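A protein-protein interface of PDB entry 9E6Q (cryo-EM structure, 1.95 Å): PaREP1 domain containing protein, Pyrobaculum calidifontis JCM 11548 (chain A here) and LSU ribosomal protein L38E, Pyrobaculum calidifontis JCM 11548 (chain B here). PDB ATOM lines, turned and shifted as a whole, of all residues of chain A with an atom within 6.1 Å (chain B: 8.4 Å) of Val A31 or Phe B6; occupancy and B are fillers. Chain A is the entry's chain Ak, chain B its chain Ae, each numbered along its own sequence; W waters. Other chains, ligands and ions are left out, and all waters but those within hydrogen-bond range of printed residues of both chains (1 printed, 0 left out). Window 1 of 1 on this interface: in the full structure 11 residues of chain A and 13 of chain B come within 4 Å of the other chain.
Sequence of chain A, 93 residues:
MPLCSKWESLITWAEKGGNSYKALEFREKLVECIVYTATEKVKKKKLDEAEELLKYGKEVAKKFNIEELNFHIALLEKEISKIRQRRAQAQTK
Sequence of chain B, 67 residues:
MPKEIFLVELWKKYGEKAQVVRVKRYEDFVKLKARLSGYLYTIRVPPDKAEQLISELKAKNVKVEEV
Hydrophobic or aromatic side chains of chain B within 4 Å of the printed part of chain A: Ile B5, Phe B6, Leu B7, Val B8 and Leu B10. Among the printed residues, no Asp or Glu carboxylate lies within 4 Å of a Lys or Arg side-chain nitrogen of the other chain.
Water W1 lies within hydrogen-bond range of the side-chain carboxylate (OE2) of Glu A68 (2.7 Å), the backbone NH (N) of Glu B9 (3.0 Å) and the backbone NH (N) of Val B8 (3.5 Å).
Among the printed residues, merely in contact across the chains: Arg A27 with Leu B7 (3.9 Å), Glu A28 with Glu B4 (3.7 Å), Glu A28 with Ile B5 (3.3 Å), Glu A28 with Leu B10 (3.8 Å), Val A31 with Phe B6 (3.7 Å), Glu A32 with Glu B4 (3.9 Å), Glu A32 with Phe B6 (3.7 Å), Val A35 with Phe B6 (3.7 Å), Tyr A36 with Phe B6 (3.5 Å), Glu A68 with Phe B6 (3.3 Å), Glu A68 with Leu B7 (3.5 Å), His A72 with Phe B6 (3.4 Å) and His A72 with Arg B44 (3.8 Å).
OE2 of Glu A28 lies close to OE2 of Glu A32, at 2.7 Å. The backbone NH (N) of Ile B5 sits at hydrogen-bond distance from the backbone carbonyl oxygen (O) of Thr B42 (2.9 Å). The side-chain amino group (NZ) of Lys A29 is in salt-bridge range of the side-chain carboxylate (OE1) of Glu A32 (3.9 Å). OE2 of Glu B4 is in salt-bridge range of NH1 of Arg B44, 2.5 Å away.
Val A31 touches just one residue of chain B: Phe B6. Printed residues of chain A within 4 Å of Phe B6: Glu A28, Val A31, Glu A32, Val A35, Tyr A36, Glu A68 and His A72. Of the printed residues of chain A, Leu B10 touches Glu A28 (3.8 Å). Printed residues of chain A within 4 Å of Ile B5: Glu A28 (3.3 Å). Of the printed residues of chain B, Glu A28 touches Glu B4, Ile B5, Phe B6, Leu B7 and Leu B10. Thr B42 touches none of the printed residues of chain A. The nearest residue of chain B that does not touch Val A31 is Leu B7 (4.1 Å). The nearest printed residue of chain A that does not touch Val B8 is Glu A28 (6.3 Å).
N of Val B8 sits at hydrogen-bond distance from OE2 of Glu A68, at 2.8 Å. The backbone NH of Phe B6 sits at hydrogen-bond distance from the side-chain carboxylate of Glu A28 (2.9 Å). The side-chain hydroxyl (OH) of Tyr A36 sits at hydrogen-bond distance from the side-chain carboxylate (OE1) of Glu B4 (2.6 Å). N of Leu B7 sits at hydrogen-bond distance from OE1 of Glu A28, at 3.1 Å.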
ATOM      1  N   PHE A  26      11.283  13.647   2.969  1.00  0.00           N
ATOM      2  CA  PHE A  26      12.428  13.144   2.223  1.00  0.00           C
ATOM      3  C   PHE A  26      13.255  12.194   3.074  1.00  0.00           C
ATOM      4  O   PHE A  26      13.827  11.229   2.561  1.00  0.00           O
ATOM      5  CB  PHE A  26      13.279  14.305   1.726  1.00  0.00           C
ATOM      6  CG  PHE A  26      12.628  15.106   0.649  1.00  0.00           C
ATOM      7  CD1 PHE A  26      11.715  14.524  -0.201  1.00  0.00           C
ATOM      8  CD2 PHE A  26      12.931  16.438   0.484  1.00  0.00           C
ATOM      9  CE1 PHE A  26      11.113  15.256  -1.191  1.00  0.00           C
ATOM     10  CE2 PHE A  26      12.334  17.173  -0.503  1.00  0.00           C
ATOM     11  CZ  PHE A  26      11.426  16.581  -1.345  1.00  0.00           C
ATOM     12  N   ARG A  27      13.318  12.448   4.377  1.00  0.00           N
ATOM     13  CA  ARG A  27      13.973  11.518   5.285  1.00  0.00           C
ATOM     14  C   ARG A  27      13.288  10.161   5.259  1.00  0.00           C
ATOM     15  O   ARG A  27      13.950   9.120   5.266  1.00  0.00           O
ATOM     16  CB  ARG A  27      13.962  12.095   6.694  1.00  0.00           C
ATOM     17  CG  ARG A  27      15.015  11.539   7.590  1.00  0.00           C
ATOM     18  CD  ARG A  27      15.146  12.379   8.832  1.00  0.00           C
ATOM     19  NE  ARG A  27      15.779  13.658   8.544  1.00  0.00           N
ATOM     20  CZ  ARG A  27      16.934  14.047   9.058  1.00  0.00           C
ATOM     21  NH1 ARG A  27      17.615  13.275   9.887  1.00  0.00           N
ATOM     22  NH2 ARG A  27      17.422  15.238   8.730  1.00  0.00           N
ATOM     23  N   GLU A  28      11.957  10.160   5.235  1.00  0.00           N
ATOM     24  CA  GLU A  28      11.211   8.916   5.119  1.00  0.00           C
ATOM     25  C   GLU A  28      11.489   8.223   3.794  1.00  0.00           C
ATOM     26  O   GLU A  28      11.636   6.999   3.744  1.00  0.00           O
ATOM     27  CB  GLU A  28       9.718   9.203   5.282  1.00  0.00           C
ATOM     28  CG  GLU A  28       8.813   8.096   4.815  1.00  0.00           C
ATOM     29  CD  GLU A  28       8.701   6.980   5.823  1.00  0.00           C
ATOM     30  OE1 GLU A  28       9.241   7.128   6.933  1.00  0.00           O
ATOM     31  OE2 GLU A  28       8.090   5.946   5.505  1.00  0.00           O
ATOM     32  N   LYS A  29      11.562   8.988   2.706  1.00  0.00           N
ATOM     33  CA  LYS A  29      11.799   8.387   1.399  1.00  0.00           C
ATOM     34  C   LYS A  29      13.187   7.772   1.318  1.00  0.00           C
ATOM     35  O   LYS A  29      13.376   6.747   0.657  1.00  0.00           O
ATOM     36  CB  LYS A  29      11.605   9.429   0.305  1.00  0.00           C
ATOM     37  CG  LYS A  29      10.196   9.953   0.227  1.00  0.00           C
ATOM     38  CD  LYS A  29       9.478   9.419  -0.975  1.00  0.00           C
ATOM     39  CE  LYS A  29       8.062   9.941  -1.043  1.00  0.00           C
ATOM     40  NZ  LYS A  29       7.089   8.828  -0.940  1.00  0.00           N
ATOM     41  N   LEU A  30      14.168   8.381   1.981  1.00  0.00           N
ATOM     42  CA  LEU A  30      15.511   7.816   1.999  1.00  0.00           C
ATOM     43  C   LEU A  30      15.517   6.444   2.657  1.00  0.00           C
ATOM     44  O   LEU A  30      16.123   5.501   2.143  1.00  0.00           O
ATOM     45  CB  LEU A  30      16.464   8.762   2.723  1.00  0.00           C
ATOM     46  CG  LEU A  30      17.824   8.194   3.105  1.00  0.00           C
ATOM     47  CD1 LEU A  30      18.606   7.861   1.860  1.00  0.00           C
ATOM     48  CD2 LEU A  30      18.582   9.184   3.956  1.00  0.00           C
ATOM     49  N   VAL A  31      14.836   6.313   3.795  1.00  0.00           N
ATOM     50  CA  VAL A  31      14.779   5.027   4.478  1.00  0.00           C
ATOM     51  C   VAL A  31      14.032   4.009   3.633  1.00  0.00           C
ATOM     52  O   VAL A  31      14.448   2.851   3.521  1.00  0.00           O
ATOM     53  CB  VAL A  31      14.139   5.185   5.867  1.00  0.00           C
ATOM     54  CG1 VAL A  31      13.980   3.835   6.523  1.00  0.00           C
ATOM     55  CG2 VAL A  31      14.978   6.093   6.724  1.00  0.00           C
ATOM     56  N   GLU A  32      12.922   4.423   3.023  1.00  0.00           N
ATOM     57  CA  GLU A  32      12.191   3.534   2.133  1.00  0.00           C
ATOM     58  C   GLU A  32      13.094   3.016   1.025  1.00  0.00           C
ATOM     59  O   GLU A  32      13.113   1.818   0.739  1.00  0.00           O
ATOM     60  CB  GLU A  32      10.985   4.258   1.539  1.00  0.00           C
ATOM     61  CG  GLU A  32       9.768   4.280   2.425  1.00  0.00           C
ATOM     62  CD  GLU A  32       8.777   5.349   2.022  1.00  0.00           C
ATOM     63  OE1 GLU A  32       8.849   5.834   0.879  1.00  0.00           O
ATOM     64  OE2 GLU A  32       7.911   5.704   2.841  1.00  0.00           O
ATOM     65  N   CYS A  33      13.878   3.905   0.416  1.00  0.00           N
ATOM     66  CA  CYS A  33      14.745   3.510  -0.688  1.00  0.00           C
ATOM     67  C   CYS A  33      15.739   2.446  -0.248  1.00  0.00           C
ATOM     68  O   CYS A  33      15.930   1.440  -0.936  1.00  0.00           O
ATOM     69  CB  CYS A  33      15.473   4.735  -1.241  1.00  0.00           C
ATOM     70  SG  CYS A  33      16.685   4.405  -2.535  1.00  0.00           S
ATOM     71  N   ILE A  34      16.368   2.639   0.907  1.00  0.00           N
ATOM     72  CA  ILE A  34      17.372   1.685   1.360  1.00  0.00           C
ATOM     73  C   ILE A  34      16.719   0.379   1.790  1.00  0.00           C
ATOM     74  O   ILE A  34      17.094  -0.701   1.327  1.00  0.00           O
ATOM     75  CB  ILE A  34      18.215   2.292   2.493  1.00  0.00           C
ATOM     76  CG1 ILE A  34      19.141   3.364   1.935  1.00  0.00           C
ATOM     77  CG2 ILE A  34      19.013   1.219   3.193  1.00  0.00           C
ATOM     78  CD1 ILE A  34      19.833   4.155   2.986  1.00  0.00           C
ATOM     79  N   VAL A  35      15.721   0.459   2.669  1.00  0.00           N
ATOM     80  CA  VAL A  35      15.149  -0.752   3.250  1.00  0.00           C
ATOM     81  C   VAL A  35      14.418  -1.564   2.190  1.00  0.00           C
ATOM     82  O   VAL A  35      14.615  -2.777   2.072  1.00  0.00           O
ATOM     83  CB  VAL A  35      14.226  -0.399   4.428  1.00  0.00           C
ATOM     84  CG1 VAL A  35      13.502  -1.638   4.906  1.00  0.00           C
ATOM     85  CG2 VAL A  35      15.032   0.219   5.551  1.00  0.00           C
ATOM     86  N   TYR A  36      13.569  -0.909   1.398  1.00  0.00           N
ATOM     87  CA  TYR A  36      12.800  -1.639   0.397  1.00  0.00           C
ATOM     88  C   TYR A  36      13.712  -2.315  -0.616  1.00  0.00           C
ATOM     89  O   TYR A  36      13.479  -3.464  -0.997  1.00  0.00           O
ATOM     90  CB  TYR A  36      11.824  -0.708  -0.316  1.00  0.00           C
ATOM     91  CG  TYR A  36      10.595  -0.338   0.475  1.00  0.00           C
ATOM     92  CD1 TYR A  36      10.133  -1.141   1.500  1.00  0.00           C
ATOM     93  CD2 TYR A  36       9.887   0.812   0.179  1.00  0.00           C
ATOM     94  CE1 TYR A  36       9.007  -0.806   2.210  1.00  0.00           C
ATOM     95  CE2 TYR A  36       8.765   1.158   0.883  1.00  0.00           C
ATOM     96  CZ  TYR A  36       8.328   0.346   1.897  1.00  0.00           C
ATOM     97  OH  TYR A  36       7.210   0.694   2.600  1.00  0.00           O
ATOM     98  N   ILE A  66      19.319   8.617  11.994  1.00  0.00           N
ATOM     99  CA  ILE A  66      18.043   7.957  11.767  1.00  0.00           C
ATOM    100  C   ILE A  66      18.110   6.632  12.515  1.00  0.00           C
ATOM    101  O   ILE A  66      18.754   5.681  12.064  1.00  0.00           O
ATOM    102  CB  ILE A  66      17.763   7.754  10.276  1.00  0.00           C
ATOM    103  CG1 ILE A  66      17.350   9.070   9.635  1.00  0.00           C
ATOM    104  CG2 ILE A  66      16.599   6.810  10.095  1.00  0.00           C
ATOM    105  CD1 ILE A  66      17.602   9.109   8.157  1.00  0.00           C
ATOM    106  N   GLU A  68      15.665   4.451  13.178  1.00  0.00           N
ATOM    107  CA  GLU A  68      14.892   3.377  12.568  1.00  0.00           C
ATOM    108  C   GLU A  68      15.666   2.680  11.462  1.00  0.00           C
ATOM    109  O   GLU A  68      15.433   1.499  11.190  1.00  0.00           O
ATOM    110  CB  GLU A  68      13.577   3.931  12.028  1.00  0.00           C
ATOM    111  CG  GLU A  68      12.677   4.536  13.094  1.00  0.00           C
ATOM    112  CD  GLU A  68      12.916   6.019  13.296  1.00  0.00           C
ATOM    113  OE1 GLU A  68      14.046   6.481  13.041  1.00  0.00           O
ATOM    114  OE2 GLU A  68      11.975   6.724  13.706  1.00  0.00           O
ATOM    115  N   LEU A  69      16.581   3.390  10.806  1.00  0.00           N
ATOM    116  CA  LEU A  69      17.403   2.761   9.782  1.00  0.00           C
ATOM    117  C   LEU A  69      18.303   1.694  10.387  1.00  0.00           C
ATOM    118  O   LEU A  69      18.464   0.613   9.813  1.00  0.00           O
ATOM    119  CB  LEU A  69      18.220   3.821   9.051  1.00  0.00           C
ATOM    120  CG  LEU A  69      18.779   3.477   7.679  1.00  0.00           C
ATOM    121  CD1 LEU A  69      17.771   2.701   6.860  1.00  0.00           C
ATOM    122  CD2 LEU A  69      19.181   4.751   6.971  1.00  0.00           C
ATOM    123  N   HIS A  72      16.240  -1.549  11.222  1.00  0.00           N
ATOM    124  CA  HIS A  72      15.893  -2.364  10.068  1.00  0.00           C
ATOM    125  C   HIS A  72      17.119  -2.977   9.408  1.00  0.00           C
ATOM    126  O   HIS A  72      17.017  -4.049   8.803  1.00  0.00           O
ATOM    127  CB  HIS A  72      15.104  -1.529   9.062  1.00  0.00           C
ATOM    128  CG  HIS A  72      13.674  -1.327   9.444  1.00  0.00           C
ATOM    129  ND1 HIS A  72      12.739  -2.337   9.383  1.00  0.00           N
ATOM    130  CD2 HIS A  72      13.020  -0.237   9.907  1.00  0.00           C
ATOM    131  CE1 HIS A  72      11.570  -1.876   9.787  1.00  0.00           C
ATOM    132  NE2 HIS A  72      11.713  -0.605  10.111  1.00  0.00           N
ATOM    133  N   LYS B   3      -0.777   2.103   3.889  1.00  0.00           N
ATOM    134  CA  LYS B   3       0.505   2.757   3.699  1.00  0.00           C
ATOM    135  C   LYS B   3       1.458   2.335   4.802  1.00  0.00           C
ATOM    136  O   LYS B   3       1.040   2.029   5.917  1.00  0.00           O
ATOM    137  CB  LYS B   3       0.359   4.277   3.700  1.00  0.00           C
ATOM    138  CG  LYS B   3      -0.458   4.809   2.557  1.00  0.00           C
ATOM    139  CD  LYS B   3      -0.392   6.306   2.499  1.00  0.00           C
ATOM    140  CE  LYS B   3      -1.480   6.861   1.625  1.00  0.00           C
ATOM    141  NZ  LYS B   3      -1.319   8.314   1.443  1.00  0.00           N
ATOM    142  N   GLU B   4       2.743   2.322   4.488  1.00  0.00           N
ATOM    143  CA  GLU B   4       3.763   1.990   5.464  1.00  0.00           C
ATOM    144  C   GLU B   4       4.649   3.197   5.715  1.00  0.00           C
ATOM    145  O   GLU B   4       5.053   3.891   4.781  1.00  0.00           O
ATOM    146  CB  GLU B   4       4.611   0.808   5.028  1.00  0.00           C
ATOM    147  CG  GLU B   4       5.623   0.406   6.072  1.00  0.00           C
ATOM    148  CD  GLU B   4       6.525  -0.720   5.624  1.00  0.00           C
ATOM    149  OE1 GLU B   4       6.569  -1.001   4.414  1.00  0.00           O
ATOM    150  OE2 GLU B   4       7.179  -1.331   6.489  1.00  0.00           O
ATOM    151  N   ILE B   5       4.929   3.443   6.988  1.00  0.00           N
ATOM    152  CA  ILE B   5       5.776   4.538   7.431  1.00  0.00           C
ATOM    153  C   ILE B   5       6.904   3.940   8.253  1.00  0.00           C
ATOM    154  O   ILE B   5       6.670   3.051   9.076  1.00  0.00           O
ATOM    155  CB  ILE B   5       4.977   5.564   8.251  1.00  0.00           C
ATOM    156  CG1 ILE B   5       3.819   6.096   7.409  1.00  0.00           C
ATOM    157  CG2 ILE B   5       5.874   6.681   8.722  1.00  0.00           C
ATOM    158  CD1 ILE B   5       3.315   7.428   7.829  1.00  0.00           C
ATOM    159  N   PHE B   6       8.125   4.405   8.016  1.00  0.00           N
ATOM    160  CA  PHE B   6       9.284   3.885   8.726  1.00  0.00           C
ATOM    161  C   PHE B   6       9.707   4.744   9.907  1.00  0.00           C
ATOM    162  O   PHE B   6      10.228   4.206  10.886  1.00  0.00           O
ATOM    163  CB  PHE B   6      10.466   3.730   7.767  1.00  0.00           C
ATOM    164  CG  PHE B   6      10.392   2.500   6.919  1.00  0.00           C
ATOM    165  CD1 PHE B   6      10.841   1.289   7.397  1.00  0.00           C
ATOM    166  CD2 PHE B   6       9.863   2.554   5.646  1.00  0.00           C
ATOM    167  CE1 PHE B   6      10.770   0.162   6.620  1.00  0.00           C
ATOM    168  CE2 PHE B   6       9.787   1.429   4.872  1.00  0.00           C
ATOM    169  CZ  PHE B   6      10.240   0.231   5.358  1.00  0.00           C
ATOM    170  N   LEU B   7       9.492   6.055   9.848  1.00  0.00           N
ATOM    171  CA  LEU B   7       9.923   6.962  10.905  1.00  0.00           C
ATOM    172  C   LEU B   7       8.830   7.117  11.949  1.00  0.00           C
ATOM    173  O   LEU B   7       7.682   7.406  11.612  1.00  0.00           O
ATOM    174  CB  LEU B   7      10.284   8.328  10.330  1.00  0.00           C
ATOM    175  CG  LEU B   7      11.314   8.328   9.206  1.00  0.00           C
ATOM    176  CD1 LEU B   7      11.566   9.743   8.739  1.00  0.00           C
ATOM    177  CD2 LEU B   7      12.597   7.662   9.649  1.00  0.00           C
ATOM    178  N   VAL B   8       9.201   6.947  13.219  1.00  0.00           N
ATOM    179  CA  VAL B   8       8.229   7.067  14.300  1.00  0.00           C
ATOM    180  C   VAL B   8       7.665   8.478  14.358  1.00  0.00           C
ATOM    181  O   VAL B   8       6.461   8.673  14.552  1.00  0.00           O
ATOM    182  CB  VAL B   8       8.863   6.661  15.643  1.00  0.00           C
ATOM    183  CG1 VAL B   8       7.914   6.950  16.772  1.00  0.00           C
ATOM    184  CG2 VAL B   8       9.222   5.201  15.636  1.00  0.00           C
ATOM    185  N   GLU B   9       8.525   9.483  14.198  1.00  0.00           N
ATOM    186  CA  GLU B   9       8.069  10.864  14.287  1.00  0.00           C
ATOM    187  C   GLU B   9       7.012  11.163  13.234  1.00  0.00           C
ATOM    188  O   GLU B   9       6.022  11.847  13.513  1.00  0.00           O
ATOM    189  CB  GLU B   9       9.260  11.809  14.151  1.00  0.00           C
ATOM    190  CG  GLU B   9       8.956  13.097  13.431  1.00  0.00           C
ATOM    191  CD  GLU B   9      10.081  14.104  13.537  1.00  0.00           C
ATOM    192  OE1 GLU B   9       9.809  15.269  13.885  1.00  0.00           O
ATOM    193  OE2 GLU B   9      11.242  13.728  13.277  1.00  0.00           O
ATOM    194  N   LEU B  10       7.199  10.649  12.021  1.00  0.00           N
ATOM    195  CA  LEU B  10       6.194  10.815  10.979  1.00  0.00           C
ATOM    196  C   LEU B  10       4.932  10.020  11.292  1.00  0.00           C
ATOM    197  O   LEU B  10       3.817  10.502  11.076  1.00  0.00           O
ATOM    198  CB  LEU B  10       6.777  10.399   9.629  1.00  0.00           C
ATOM    199  CG  LEU B  10       5.891  10.646   8.411  1.00  0.00           C
ATOM    200  CD1 LEU B  10       5.346  12.065   8.410  1.00  0.00           C
ATOM    201  CD2 LEU B  10       6.636  10.344   7.120  1.00  0.00           C
ATOM    202  N   TRP B  11       5.084   8.795  11.797  1.00  0.00           N
ATOM    203  CA  TRP B  11       3.919   7.947  12.026  1.00  0.00           C
ATOM    204  C   TRP B  11       3.026   8.510  13.120  1.00  0.00           C
ATOM    205  O   TRP B  11       1.802   8.349  13.073  1.00  0.00           O
ATOM    206  CB  TRP B  11       4.354   6.525  12.377  1.00  0.00           C
ATOM    207  CG  TRP B  11       3.195   5.609  12.639  1.00  0.00           C
ATOM    208  CD1 TRP B  11       2.517   4.869  11.724  1.00  0.00           C
ATOM    209  CD2 TRP B  11       2.572   5.353  13.900  1.00  0.00           C
ATOM    210  NE1 TRP B  11       1.514   4.165  12.332  1.00  0.00           N
ATOM    211  CE2 TRP B  11       1.528   4.443  13.672  1.00  0.00           C
ATOM    212  CE3 TRP B  11       2.799   5.800  15.202  1.00  0.00           C
ATOM    213  CZ2 TRP B  11       0.713   3.976  14.691  1.00  0.00           C
ATOM    214  CZ3 TRP B  11       1.991   5.336  16.211  1.00  0.00           C
ATOM    215  CH2 TRP B  11       0.961   4.432  15.952  1.00  0.00           C
ATOM    216  N   THR B  42       0.778   1.694   8.820  1.00  0.00           N
ATOM    217  CA  THR B  42       1.500   0.670   9.565  1.00  0.00           C
ATOM    218  C   THR B  42       2.944   1.093   9.785  1.00  0.00           C
ATOM    219  O   THR B  42       3.581   1.642   8.885  1.00  0.00           O
ATOM    220  CB  THR B  42       1.471  -0.672   8.823  1.00  0.00           C
ATOM    221  OG1 THR B  42       0.127  -1.149   8.734  1.00  0.00           O
ATOM    222  CG2 THR B  42       2.304  -1.708   9.539  1.00  0.00           C
ATOM    223  N   ILE B  43       3.457   0.848  10.987  1.00  0.00           N
ATOM    224  CA  ILE B  43       4.876   1.011  11.274  1.00  0.00           C
ATOM    225  C   ILE B  43       5.365  -0.207  12.043  1.00  0.00           C
ATOM    226  O   ILE B  43       4.678  -0.715  12.933  1.00  0.00           O
ATOM    227  CB  ILE B  43       5.168   2.306  12.057  1.00  0.00           C
ATOM    228  CG1 ILE B  43       6.668   2.443  12.308  1.00  0.00           C
ATOM    229  CG2 ILE B  43       4.410   2.333  13.363  1.00  0.00           C
ATOM    230  CD1 ILE B  43       7.135   3.853  12.382  1.00  0.00           C
ATOM    231  N   ARG B  44       6.546  -0.686  11.682  1.00  0.00           N
ATOM    232  CA  ARG B  44       7.231  -1.740  12.413  1.00  0.00           C
ATOM    233  C   ARG B  44       8.268  -1.111  13.331  1.00  0.00           C
ATOM    234  O   ARG B  44       9.095  -0.315  12.883  1.00  0.00           O
ATOM    235  CB  ARG B  44       7.900  -2.722  11.455  1.00  0.00           C
ATOM    236  CG  ARG B  44       6.947  -3.720  10.852  1.00  0.00           C
ATOM    237  CD  ARG B  44       7.013  -3.714   9.343  1.00  0.00           C
ATOM    238  NE  ARG B  44       8.095  -4.553   8.847  1.00  0.00           N
ATOM    239  CZ  ARG B  44       8.895  -4.228   7.844  1.00  0.00           C
ATOM    240  NH1 ARG B  44       8.734  -3.106   7.166  1.00  0.00           N
ATOM    241  NH2 ARG B  44       9.883  -5.051   7.509  1.00  0.00           N
ATOM    242  N   VAL B  45       8.220  -1.467  14.608  1.00  0.00           N
ATOM    243  CA  VAL B  45       9.095  -0.859  15.607  1.00  0.00           C
ATOM    244  C   VAL B  45       9.705  -1.967  16.453  1.00  0.00           C
ATOM    245  O   VAL B  45       9.191  -3.094  16.487  1.00  0.00           O
ATOM    246  CB  VAL B  45       8.333   0.153  16.492  1.00  0.00           C
ATOM    247  CG1 VAL B  45       7.858   1.329  15.667  1.00  0.00           C
ATOM    248  CG2 VAL B  45       7.170  -0.517  17.161  1.00  0.00           C
ATOM    249  N   PRO B  46      10.813  -1.687  17.135  1.00  0.00           N
ATOM    250  CA  PRO B  46      11.301  -2.627  18.137  1.00  0.00           C
ATOM    251  C   PRO B  46      10.292  -2.773  19.256  1.00  0.00           C
ATOM    252  O   PRO B  46       9.522  -1.838  19.547  1.00  0.00           O
ATOM    253  CB  PRO B  46      12.601  -1.982  18.633  1.00  0.00           C
ATOM    254  CG  PRO B  46      12.878  -0.857  17.770  1.00  0.00           C
ATOM    255  CD  PRO B  46      11.712  -0.540  16.937  1.00  0.00           C
HETATM  256  O   HOH W   1      11.559   9.383  14.015  1.00  0.00           O
